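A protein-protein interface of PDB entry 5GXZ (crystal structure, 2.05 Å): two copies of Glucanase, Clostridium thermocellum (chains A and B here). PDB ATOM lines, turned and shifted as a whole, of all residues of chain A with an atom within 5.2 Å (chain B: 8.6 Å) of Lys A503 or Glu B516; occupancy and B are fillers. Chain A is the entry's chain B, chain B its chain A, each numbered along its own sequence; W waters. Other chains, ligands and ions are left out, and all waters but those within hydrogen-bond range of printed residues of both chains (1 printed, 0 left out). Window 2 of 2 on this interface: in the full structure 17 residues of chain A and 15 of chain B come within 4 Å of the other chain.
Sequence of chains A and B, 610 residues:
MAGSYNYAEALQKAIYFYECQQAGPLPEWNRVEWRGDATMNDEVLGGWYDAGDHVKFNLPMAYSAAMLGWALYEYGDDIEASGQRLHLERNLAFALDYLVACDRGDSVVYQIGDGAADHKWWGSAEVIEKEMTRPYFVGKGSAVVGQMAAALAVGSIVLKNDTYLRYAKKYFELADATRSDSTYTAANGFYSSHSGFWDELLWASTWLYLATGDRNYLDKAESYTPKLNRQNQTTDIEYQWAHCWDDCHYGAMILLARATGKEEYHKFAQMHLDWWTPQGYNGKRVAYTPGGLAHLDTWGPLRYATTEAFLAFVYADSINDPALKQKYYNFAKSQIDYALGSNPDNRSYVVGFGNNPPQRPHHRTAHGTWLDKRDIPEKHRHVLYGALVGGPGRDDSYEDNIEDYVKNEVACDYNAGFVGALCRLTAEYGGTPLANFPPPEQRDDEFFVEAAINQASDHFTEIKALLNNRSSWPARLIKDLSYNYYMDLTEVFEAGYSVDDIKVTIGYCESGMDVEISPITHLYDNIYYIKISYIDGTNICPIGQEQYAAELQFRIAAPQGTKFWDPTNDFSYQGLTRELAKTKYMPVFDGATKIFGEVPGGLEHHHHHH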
ATOM      1  N   VAL A 499      17.577   1.066  25.559  1.00  0.00           N
ATOM      2  CA  VAL A 499      17.305  -0.068  24.686  1.00  0.00           C
ATOM      3  C   VAL A 499      18.249  -0.069  23.490  1.00  0.00           C
ATOM      4  O   VAL A 499      18.706  -1.127  23.046  1.00  0.00           O
ATOM      5  CB  VAL A 499      15.831  -0.084  24.220  1.00  0.00           C
ATOM      6  CG1 VAL A 499      15.638  -1.022  23.036  1.00  0.00           C
ATOM      7  CG2 VAL A 499      14.938  -0.508  25.369  1.00  0.00           C
ATOM      8  N   ASP A 501      21.205   0.939  23.402  1.00  0.00           N
ATOM      9  CA  ASP A 501      22.499   0.468  23.895  1.00  0.00           C
ATOM     10  C   ASP A 501      22.644  -1.059  23.784  1.00  0.00           C
ATOM     11  O   ASP A 501      23.729  -1.605  23.987  1.00  0.00           O
ATOM     12  CB  ASP A 501      22.696   0.923  25.349  1.00  0.00           C
ATOM     13  CG  ASP A 501      22.859   2.436  25.482  1.00  0.00           C
ATOM     14  OD1 ASP A 501      23.715   3.012  24.778  1.00  0.00           O
ATOM     15  OD2 ASP A 501      22.136   3.063  26.288  1.00  0.00           O
ATOM     16  N   ILE A 502      21.542  -1.743  23.475  1.00  0.00           N
ATOM     17  CA  ILE A 502      21.497  -3.198  23.318  1.00  0.00           C
ATOM     18  C   ILE A 502      21.250  -3.588  21.852  1.00  0.00           C
ATOM     19  O   ILE A 502      20.267  -3.166  21.236  1.00  0.00           O
ATOM     20  CB  ILE A 502      20.402  -3.821  24.219  1.00  0.00           C
ATOM     21  CG1 ILE A 502      20.387  -3.176  25.613  1.00  0.00           C
ATOM     22  CG2 ILE A 502      20.554  -5.334  24.288  1.00  0.00           C
ATOM     23  CD1 ILE A 502      21.629  -3.428  26.476  1.00  0.00           C
ATOM     24  N   LYS A 503      22.158  -4.396  21.313  1.00  0.00           N
ATOM     25  CA  LYS A 503      22.164  -4.756  19.888  1.00  0.00           C
ATOM     26  C   LYS A 503      21.968  -6.264  19.661  1.00  0.00           C
ATOM     27  O   LYS A 503      22.542  -7.077  20.388  1.00  0.00           O
ATOM     28  CB  LYS A 503      23.500  -4.327  19.274  1.00  0.00           C
ATOM     29  CG  LYS A 503      23.830  -4.973  17.933  1.00  0.00           C
ATOM     30  CD  LYS A 503      25.340  -5.093  17.712  1.00  0.00           C
ATOM     31  CE  LYS A 503      25.844  -4.112  16.678  1.00  0.00           C
ATOM     32  NZ  LYS A 503      25.384  -2.723  16.924  1.00  0.00           N
ATOM     33  N   VAL A 504      21.196  -6.628  18.640  1.00  0.00           N
ATOM     34  CA  VAL A 504      20.941  -8.042  18.328  1.00  0.00           C
ATOM     35  C   VAL A 504      21.763  -8.509  17.123  1.00  0.00           C
ATOM     36  O   VAL A 504      21.650  -7.946  16.040  1.00  0.00           O
ATOM     37  CB  VAL A 504      19.442  -8.313  18.048  1.00  0.00           C
ATOM     38  CG1 VAL A 504      19.191  -9.787  17.753  1.00  0.00           C
ATOM     39  CG2 VAL A 504      18.588  -7.859  19.224  1.00  0.00           C
ATOM     40  N   THR A 505      22.563  -9.557  17.317  1.00  0.00           N
ATOM     41  CA  THR A 505      23.360 -10.148  16.240  1.00  0.00           C
ATOM     42  C   THR A 505      23.182 -11.678  16.149  1.00  0.00           C
ATOM     43  O   THR A 505      22.654 -12.315  17.070  1.00  0.00           O
ATOM     44  CB  THR A 505      24.856  -9.804  16.387  1.00  0.00           C
ATOM     45  OG1 THR A 505      25.297 -10.189  17.692  1.00  0.00           O
ATOM     46  CG2 THR A 505      25.118  -8.314  16.195  1.00  0.00           C
ATOM     47  N   ILE A 520      14.142  -5.743  19.354  1.00  0.00           N
ATOM     48  CA  ILE A 520      13.812  -5.912  20.769  1.00  0.00           C
ATOM     49  C   ILE A 520      12.505  -5.172  21.017  1.00  0.00           C
ATOM     50  O   ILE A 520      12.323  -4.044  20.556  1.00  0.00           O
ATOM     51  CB  ILE A 520      14.924  -5.392  21.699  1.00  0.00           C
ATOM     52  CG1 ILE A 520      16.174  -6.257  21.550  1.00  0.00           C
ATOM     53  CG2 ILE A 520      14.466  -5.368  23.160  1.00  0.00           C
ATOM     54  CD1 ILE A 520      17.415  -5.646  22.153  1.00  0.00           C
ATOM     55  N   ARG A 555      23.052 -13.368  19.647  1.00  0.00           N
ATOM     56  CA  ARG A 555      23.688 -12.599  20.713  1.00  0.00           C
ATOM     57  C   ARG A 555      22.903 -11.316  20.947  1.00  0.00           C
ATOM     58  O   ARG A 555      22.443 -10.656  20.012  1.00  0.00           O
ATOM     59  CB  ARG A 555      25.147 -12.266  20.364  1.00  0.00           C
ATOM     60  CG  ARG A 555      25.908 -11.474  21.428  1.00  0.00           C
ATOM     61  CD  ARG A 555      27.312 -11.074  20.960  1.00  0.00           C
ATOM     62  NE  ARG A 555      28.177 -12.242  20.833  1.00  0.00           N
ATOM     63  CZ  ARG A 555      29.492 -12.206  20.631  1.00  0.00           C
ATOM     64  NH1 ARG A 555      30.123 -11.046  20.521  1.00  0.00           N
ATOM     65  NH2 ARG A 555      30.185 -13.336  20.546  1.00  0.00           N
ATOM     66  N   ILE A 556      22.725 -10.996  22.224  1.00  0.00           N
ATOM     67  CA  ILE A 556      22.117  -9.744  22.651  1.00  0.00           C
ATOM     68  C   ILE A 556      23.181  -9.115  23.544  1.00  0.00           C
ATOM     69  O   ILE A 556      23.579  -9.700  24.558  1.00  0.00           O
ATOM     70  CB  ILE A 556      20.820 -10.006  23.442  1.00  0.00           C
ATOM     71  CG1 ILE A 556      19.856 -10.851  22.603  1.00  0.00           C
ATOM     72  CG2 ILE A 556      20.170  -8.699  23.877  1.00  0.00           C
ATOM     73  CD1 ILE A 556      18.846 -11.611  23.437  1.00  0.00           C
ATOM     74  N   ALA A 557      23.662  -7.944  23.131  1.00  0.00           N
ATOM     75  CA  ALA A 557      24.853  -7.353  23.729  1.00  0.00           C
ATOM     76  C   ALA A 557      24.694  -5.889  24.120  1.00  0.00           C
ATOM     77  O   ALA A 557      24.120  -5.080  23.376  1.00  0.00           O
ATOM     78  CB  ALA A 557      26.055  -7.499  22.804  1.00  0.00           C
ATOM     79  N   ALA A 558      25.225  -5.588  25.303  1.00  0.00           N
ATOM     80  CA  ALA A 558      25.448  -4.212  25.745  1.00  0.00           C
ATOM     81  C   ALA A 558      26.775  -3.739  25.129  1.00  0.00           C
ATOM     82  O   ALA A 558      27.537  -4.577  24.625  1.00  0.00           O
ATOM     83  CB  ALA A 558      25.488  -4.159  27.267  1.00  0.00           C
ATOM     84  N   LEU B 481      34.181  -4.097   9.746  1.00  0.00           N
ATOM     85  CA  LEU B 481      33.947  -4.365   8.327  1.00  0.00           C
ATOM     86  C   LEU B 481      32.453  -4.412   8.049  1.00  0.00           C
ATOM     87  O   LEU B 481      31.708  -5.007   8.819  1.00  0.00           O
ATOM     88  CB  LEU B 481      34.599  -5.688   7.911  1.00  0.00           C
ATOM     89  CG  LEU B 481      36.101  -5.701   7.613  1.00  0.00           C
ATOM     90  CD1 LEU B 481      36.495  -7.128   7.276  1.00  0.00           C
ATOM     91  CD2 LEU B 481      36.436  -4.781   6.435  1.00  0.00           C
ATOM     92  N   SER B 482      32.021  -3.803   6.951  1.00  0.00           N
ATOM     93  CA  SER B 482      30.650  -3.956   6.495  1.00  0.00           C
ATOM     94  C   SER B 482      30.580  -3.809   4.983  1.00  0.00           C
ATOM     95  O   SER B 482      31.546  -3.397   4.330  1.00  0.00           O
ATOM     96  CB  SER B 482      29.716  -2.940   7.161  1.00  0.00           C
ATOM     97  OG  SER B 482      30.040  -1.629   6.725  1.00  0.00           O
ATOM     98  N   TYR B 483      29.441  -4.190   4.419  1.00  0.00           N
ATOM     99  CA  TYR B 483      29.186  -3.902   3.012  1.00  0.00           C
ATOM    100  C   TYR B 483      27.707  -3.605   2.830  1.00  0.00           C
ATOM    101  O   TYR B 483      26.890  -3.956   3.689  1.00  0.00           O
ATOM    102  CB  TYR B 483      29.650  -5.044   2.105  1.00  0.00           C
ATOM    103  CG  TYR B 483      28.967  -6.382   2.327  1.00  0.00           C
ATOM    104  CD1 TYR B 483      27.770  -6.689   1.690  1.00  0.00           C
ATOM    105  CD2 TYR B 483      29.531  -7.349   3.163  1.00  0.00           C
ATOM    106  CE1 TYR B 483      27.154  -7.928   1.881  1.00  0.00           C
ATOM    107  CE2 TYR B 483      28.907  -8.583   3.372  1.00  0.00           C
ATOM    108  CZ  TYR B 483      27.723  -8.868   2.709  1.00  0.00           C
ATOM    109  OH  TYR B 483      27.071 -10.071   2.891  1.00  0.00           O
ATOM    110  N   VAL B 504      13.489  -8.760   4.919  1.00  0.00           N
ATOM    111  CA  VAL B 504      14.867  -9.248   4.864  1.00  0.00           C
ATOM    112  C   VAL B 504      15.019 -10.441   5.802  1.00  0.00           C
ATOM    113  O   VAL B 504      14.756 -10.341   6.999  1.00  0.00           O
ATOM    114  CB  VAL B 504      15.898  -8.163   5.276  1.00  0.00           C
ATOM    115  CG1 VAL B 504      17.347  -8.672   5.143  1.00  0.00           C
ATOM    116  CG2 VAL B 504      15.720  -6.913   4.440  1.00  0.00           C
ATOM    117  N   ILE B 506      17.506 -14.295   6.489  1.00  0.00           N
ATOM    118  CA  ILE B 506      18.816 -14.917   6.328  1.00  0.00           C
ATOM    119  C   ILE B 506      18.619 -16.410   6.078  1.00  0.00           C
ATOM    120  O   ILE B 506      17.828 -17.073   6.763  1.00  0.00           O
ATOM    121  CB  ILE B 506      19.665 -14.682   7.596  1.00  0.00           C
ATOM    122  CG1 ILE B 506      20.057 -13.207   7.697  1.00  0.00           C
ATOM    123  CG2 ILE B 506      20.922 -15.519   7.602  1.00  0.00           C
ATOM    124  CD1 ILE B 506      20.262 -12.767   9.134  1.00  0.00           C
ATOM    125  N   CYS B 509      24.261 -18.198   7.836  1.00  0.00           N
ATOM    126  CA  CYS B 509      25.256 -17.293   8.406  1.00  0.00           C
ATOM    127  C   CYS B 509      26.350 -18.151   8.984  1.00  0.00           C
ATOM    128  O   CYS B 509      26.120 -18.906   9.935  1.00  0.00           O
ATOM    129  CB  CYS B 509      24.732 -16.458   9.576  1.00  0.00           C
ATOM    130  SG  CYS B 509      23.057 -15.933   9.372  1.00  0.00           S
ATOM    131  N   MET B 513      30.869 -15.938  13.034  1.00  0.00           N
ATOM    132  CA  MET B 513      30.985 -14.611  12.437  1.00  0.00           C
ATOM    133  C   MET B 513      29.814 -13.728  12.904  1.00  0.00           C
ATOM    134  O   MET B 513      28.778 -13.650  12.232  1.00  0.00           O
ATOM    135  CB  MET B 513      31.025 -14.698  10.902  1.00  0.00           C
ATOM    136  CG  MET B 513      32.169 -15.519  10.297  1.00  0.00           C
ATOM    137  SD  MET B 513      33.841 -14.970  10.707  1.00  0.00           S
ATOM    138  CE  MET B 513      33.617 -13.196  10.710  1.00  0.00           C
ATOM    139  N   ASP B 514      29.990 -13.064  14.043  1.00  0.00           N
ATOM    140  CA  ASP B 514      28.994 -12.170  14.643  1.00  0.00           C
ATOM    141  C   ASP B 514      28.596 -11.093  13.642  1.00  0.00           C
ATOM    142  O   ASP B 514      29.423 -10.265  13.246  1.00  0.00           O
ATOM    143  CB  ASP B 514      29.575 -11.570  15.934  1.00  0.00           C
ATOM    144  CG  ASP B 514      28.522 -10.932  16.846  1.00  0.00           C
ATOM    145  OD1 ASP B 514      27.333 -11.315  16.786  1.00  0.00           O
ATOM    146  OD2 ASP B 514      28.886 -10.041  17.655  1.00  0.00           O
ATOM    147  N   VAL B 515      27.345 -11.135  13.191  1.00  0.00           N
ATOM    148  CA  VAL B 515      26.909 -10.283  12.095  1.00  0.00           C
ATOM    149  C   VAL B 515      25.567  -9.638  12.397  1.00  0.00           C
ATOM    150  O   VAL B 515      24.722 -10.199  13.090  1.00  0.00           O
ATOM    151  CB  VAL B 515      26.869 -11.034  10.731  1.00  0.00           C
ATOM    152  CG1 VAL B 515      25.753 -12.063  10.675  1.00  0.00           C
ATOM    153  CG2 VAL B 515      26.714 -10.075   9.561  1.00  0.00           C
ATOM    154  N   GLU B 516      25.377  -8.434  11.886  1.00  0.00           N
ATOM    155  CA  GLU B 516      24.039  -7.884  11.851  1.00  0.00           C
ATOM    156  C   GLU B 516      23.719  -7.315  10.484  1.00  0.00           C
ATOM    157  O   GLU B 516      24.610  -7.024   9.692  1.00  0.00           O
ATOM    158  CB  GLU B 516      23.876  -6.825  12.936  1.00  0.00           C
ATOM    159  CG  GLU B 516      24.712  -5.583  12.747  1.00  0.00           C
ATOM    160  CD  GLU B 516      23.947  -4.362  13.220  1.00  0.00           C
ATOM    161  OE1 GLU B 516      22.850  -4.107  12.677  1.00  0.00           O
ATOM    162  OE2 GLU B 516      24.436  -3.668  14.131  1.00  0.00           O
ATOM    163  N   ILE B 517      22.430  -7.141  10.218  1.00  0.00           N
ATOM    164  CA  ILE B 517      21.992  -6.556   8.959  1.00  0.00           C
ATOM    165  C   ILE B 517      21.029  -5.441   9.319  1.00  0.00           C
ATOM    166  O   ILE B 517      20.102  -5.660  10.082  1.00  0.00           O
ATOM    167  CB  ILE B 517      21.251  -7.588   8.084  1.00  0.00           C
ATOM    168  CG1 ILE B 517      22.043  -8.903   8.046  1.00  0.00           C
ATOM    169  CG2 ILE B 517      20.979  -7.014   6.684  1.00  0.00           C
ATOM    170  CD1 ILE B 517      21.528  -9.927   7.048  1.00  0.00           C
ATOM    171  N   SER B 518      21.269  -4.254   8.775  1.00  0.00           N
ATOM    172  CA  SER B 518      20.463  -3.077   9.026  1.00  0.00           C
ATOM    173  C   SER B 518      19.065  -3.281   8.456  1.00  0.00           C
ATOM    174  O   SER B 518      18.881  -4.112   7.559  1.00  0.00           O
ATOM    175  CB  SER B 518      21.090  -1.873   8.325  1.00  0.00           C
ATOM    176  OG  SER B 518      20.943  -1.981   6.918  1.00  0.00           O
ATOM    177  N   PRO B 519      18.083  -2.510   8.960  1.00  0.00           N
ATOM    178  CA  PRO B 519      16.812  -2.428   8.247  1.00  0.00           C
ATOM    179  C   PRO B 519      17.060  -1.827   6.862  1.00  0.00           C
ATOM    180  O   PRO B 519      18.117  -1.244   6.629  1.00  0.00           O
ATOM    181  CB  PRO B 519      15.958  -1.486   9.114  1.00  0.00           C
ATOM    182  CG  PRO B 519      16.869  -0.947  10.198  1.00  0.00           C
ATOM    183  CD  PRO B 519      18.052  -1.869  10.288  1.00  0.00           C
ATOM    184  N   ILE B 530      20.770  -2.196   2.362  1.00  0.00           N
ATOM    185  CA  ILE B 530      20.912  -2.848   3.650  1.00  0.00           C
ATOM    186  C   ILE B 530      22.401  -2.965   3.846  1.00  0.00           C
ATOM    187  O   ILE B 530      23.146  -3.137   2.874  1.00  0.00           O
ATOM    188  CB  ILE B 530      20.222  -4.233   3.735  1.00  0.00           C
ATOM    189  CG1 ILE B 530      20.781  -5.194   2.683  1.00  0.00           C
ATOM    190  CG2 ILE B 530      18.692  -4.067   3.732  1.00  0.00           C
ATOM    191  CD1 ILE B 530      20.419  -6.650   2.914  1.00  0.00           C
ATOM    192  N   LYS B 531      22.811  -2.831   5.100  1.00  0.00           N
ATOM    193  CA  LYS B 531      24.219  -2.896   5.436  1.00  0.00           C
ATOM    194  C   LYS B 531      24.384  -4.151   6.258  1.00  0.00           C
ATOM    195  O   LYS B 531      23.685  -4.350   7.260  1.00  0.00           O
ATOM    196  CB  LYS B 531      24.686  -1.677   6.240  1.00  0.00           C
ATOM    197  CG  LYS B 531      26.073  -1.875   6.868  1.00  0.00           C
ATOM    198  CD  LYS B 531      26.586  -0.644   7.628  1.00  0.00           C
ATOM    199  CE  LYS B 531      26.952   0.507   6.693  1.00  0.00           C
ATOM    200  NZ  LYS B 531      28.017   0.110   5.721  1.00  0.00           N
ATOM    201  N   ILE B 532      25.314  -4.970   5.786  1.00  0.00           N
ATOM    202  CA  ILE B 532      25.747  -6.163   6.474  1.00  0.00           C
ATOM    203  C   ILE B 532      26.988  -5.785   7.268  1.00  0.00           C
ATOM    204  O   ILE B 532      27.997  -5.416   6.675  1.00  0.00           O
ATOM    205  CB  ILE B 532      26.067  -7.310   5.492  1.00  0.00           C
ATOM    206  CG1 ILE B 532      24.795  -7.820   4.802  1.00  0.00           C
ATOM    207  CG2 ILE B 532      26.686  -8.506   6.233  1.00  0.00           C
ATOM    208  CD1 ILE B 532      24.248  -6.946   3.674  1.00  0.00           C
ATOM    209  N   SER B 533      26.923  -5.902   8.589  1.00  0.00           N
ATOM    210  CA  SER B 533      28.057  -5.529   9.439  1.00  0.00           C
ATOM    211  C   SER B 533      28.577  -6.651  10.308  1.00  0.00           C
ATOM    212  O   SER B 533      27.806  -7.289  11.029  1.00  0.00           O
ATOM    213  CB  SER B 533      27.699  -4.367  10.366  1.00  0.00           C
ATOM    214  OG  SER B 533      27.327  -3.260   9.578  1.00  0.00           O
ATOM    215  N   TYR B 534      29.884  -6.873  10.233  1.00  0.00           N
ATOM    216  CA  TYR B 534      30.531  -7.861  11.084  1.00  0.00           C
ATOM    217  C   TYR B 534      31.106  -7.144  12.301  1.00  0.00           C
ATOM    218  O   TYR B 534      31.932  -6.237  12.161  1.00  0.00           O
ATOM    219  CB  TYR B 534      31.588  -8.664  10.309  1.00  0.00           C
ATOM    220  CG  TYR B 534      30.935  -9.612   9.335  1.00  0.00           C
ATOM    221  CD1 TYR B 534      30.482 -10.874   9.743  1.00  0.00           C
ATOM    222  CD2 TYR B 534      30.711  -9.222   8.013  1.00  0.00           C
ATOM    223  CE1 TYR B 534      29.845 -11.736   8.849  1.00  0.00           C
ATOM    224  CE2 TYR B 534      30.072 -10.062   7.120  1.00  0.00           C
ATOM    225  CZ  TYR B 534      29.638 -11.310   7.540  1.00  0.00           C
ATOM    226  OH  TYR B 534      29.027 -12.123   6.606  1.00  0.00           O
ATOM    227  N   ILE B 535      30.601  -7.511  13.476  1.00  0.00           N
ATOM    228  CA  ILE B 535      30.963  -6.837  14.719  1.00  0.00           C
ATOM    229  C   ILE B 535      32.447  -7.008  15.015  1.00  0.00           C
ATOM    230  O   ILE B 535      33.130  -6.021  15.296  1.00  0.00           O
ATOM    231  CB  ILE B 535      30.095  -7.294  15.914  1.00  0.00           C
ATOM    232  CG1 ILE B 535      28.602  -7.076  15.620  1.00  0.00           C
ATOM    233  CG2 ILE B 535      30.501  -6.581  17.189  1.00  0.00           C
ATOM    234  CD1 ILE B 535      28.226  -5.812  14.876  1.00  0.00           C
ATOM    235  N   ASP B 536      32.952  -8.237  14.937  1.00  0.00           N
ATOM    236  CA  ASP B 536      34.403  -8.427  15.039  1.00  0.00           C
ATOM    237  C   ASP B 536      34.981  -8.914  13.714  1.00  0.00           C
ATOM    238  O   ASP B 536      35.241 -10.097  13.554  1.00  0.00           O
ATOM    239  CB  ASP B 536      34.763  -9.380  16.178  1.00  0.00           C
ATOM    240  CG  ASP B 536      36.270  -9.475  16.414  1.00  0.00           C
ATOM    241  OD1 ASP B 536      37.065  -8.793  15.723  1.00  0.00           O
ATOM    242  OD2 ASP B 536      36.671 -10.236  17.318  1.00  0.00           O
ATOM    243  N   LEU B 552      27.467 -15.248   3.942  1.00  0.00           N
ATOM    244  CA  LEU B 552      26.118 -14.920   4.379  1.00  0.00           C
ATOM    245  C   LEU B 552      25.184 -15.122   3.201  1.00  0.00           C
ATOM    246  O   LEU B 552      25.489 -14.669   2.094  1.00  0.00           O
ATOM    247  CB  LEU B 552      26.034 -13.446   4.788  1.00  0.00           C
ATOM    248  CG  LEU B 552      24.653 -12.976   5.265  1.00  0.00           C
ATOM    249  CD1 LEU B 552      24.317 -13.595   6.604  1.00  0.00           C
ATOM    250  CD2 LEU B 552      24.590 -11.450   5.365  1.00  0.00           C
HETATM  251  O   HOH W   1      31.611  -9.860  17.974  1.00  0.00           O
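Water W1 lies within hydrogen-bond range of the side-chain carboxylate of Asp B514 and the guanidinium group of Arg A555.
1 position is printed for both chains. Of the 8 pairs that touch across the chains among the printed residues, none has its exchanged pair printed and touching as well.
Printed residues of chain A that touch a printed residue of chain B: Lys A503, Val A504, Thr A505 and Arg A555. Hydrophobic or aromatic side chains of chain B within 4 Å of the printed part of chain A: Ile B535. Among the printed residues, Asp or Glu carboxylates within 4 Å of a Lys or Arg side-chain nitrogen of the other chain: Lys A503 with Glu B516 and Arg A555 with Asp B514.
The side-chain hydroxyl of Thr A505 lies within hydrogen-bond range of the side-chain carboxylate of Asp B514. The guanidinium group of Arg A555 lies within salt-bridge range of the side-chain carboxylate of Asp B514. NZ of Lys A503 is in salt-bridge range of OE2 of Glu B516, at 3.1 Å.
Lys A503 touches Ile B535 (CE to CD1, 3.4 Å). CB of Glu B516 touches O of Val A504, at 3.98 Å. O of Val B515 touches CB of Thr A505, at 3.3 Å. Thr A505 touches Glu B516 (CG2 to CB, 3.8 Å). CG2 of Thr A505 touches CG1 of Ile B535 (3.7 Å).
Lys A503 touches just these residues of chain B: Glu B516 (2.9 Å) and Ile B535 (3.4 Å). Of the printed residues of chain A, Glu B516 touches Lys A503, Val A504 and Thr A505. Of the printed residues of chain B, Val A504 touches Glu B516 (3.98 Å). Of the printed residues of chain A, Val B515 touches Thr A505 (3.3 Å). Of the printed residues of chain B, Thr A505 touches Asp B514, Val B515, Glu B516 and Ile B535. Printed residues of chain A within 4 Å of Ile B535: Lys A503 and Thr A505. Of the printed residues of chain B, Arg A555 touches Asp B514 (3.3 Å).
O of Asp B514 lies within hydrogen-bond range of N of Ile B535 (3.0 Å). The backbone carbonyl oxygen (O) of Glu B516 sits at hydrogen-bond distance from the backbone NH (N) of Ser B533. The backbone NH (N) of Lys A503 is in hydrogen-bond range of the backbone carbonyl oxygen (O) of Ala A557 (2.9 Å). O of Thr A505 is in hydrogen-bond range of N of Arg A555 (2.8 Å).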
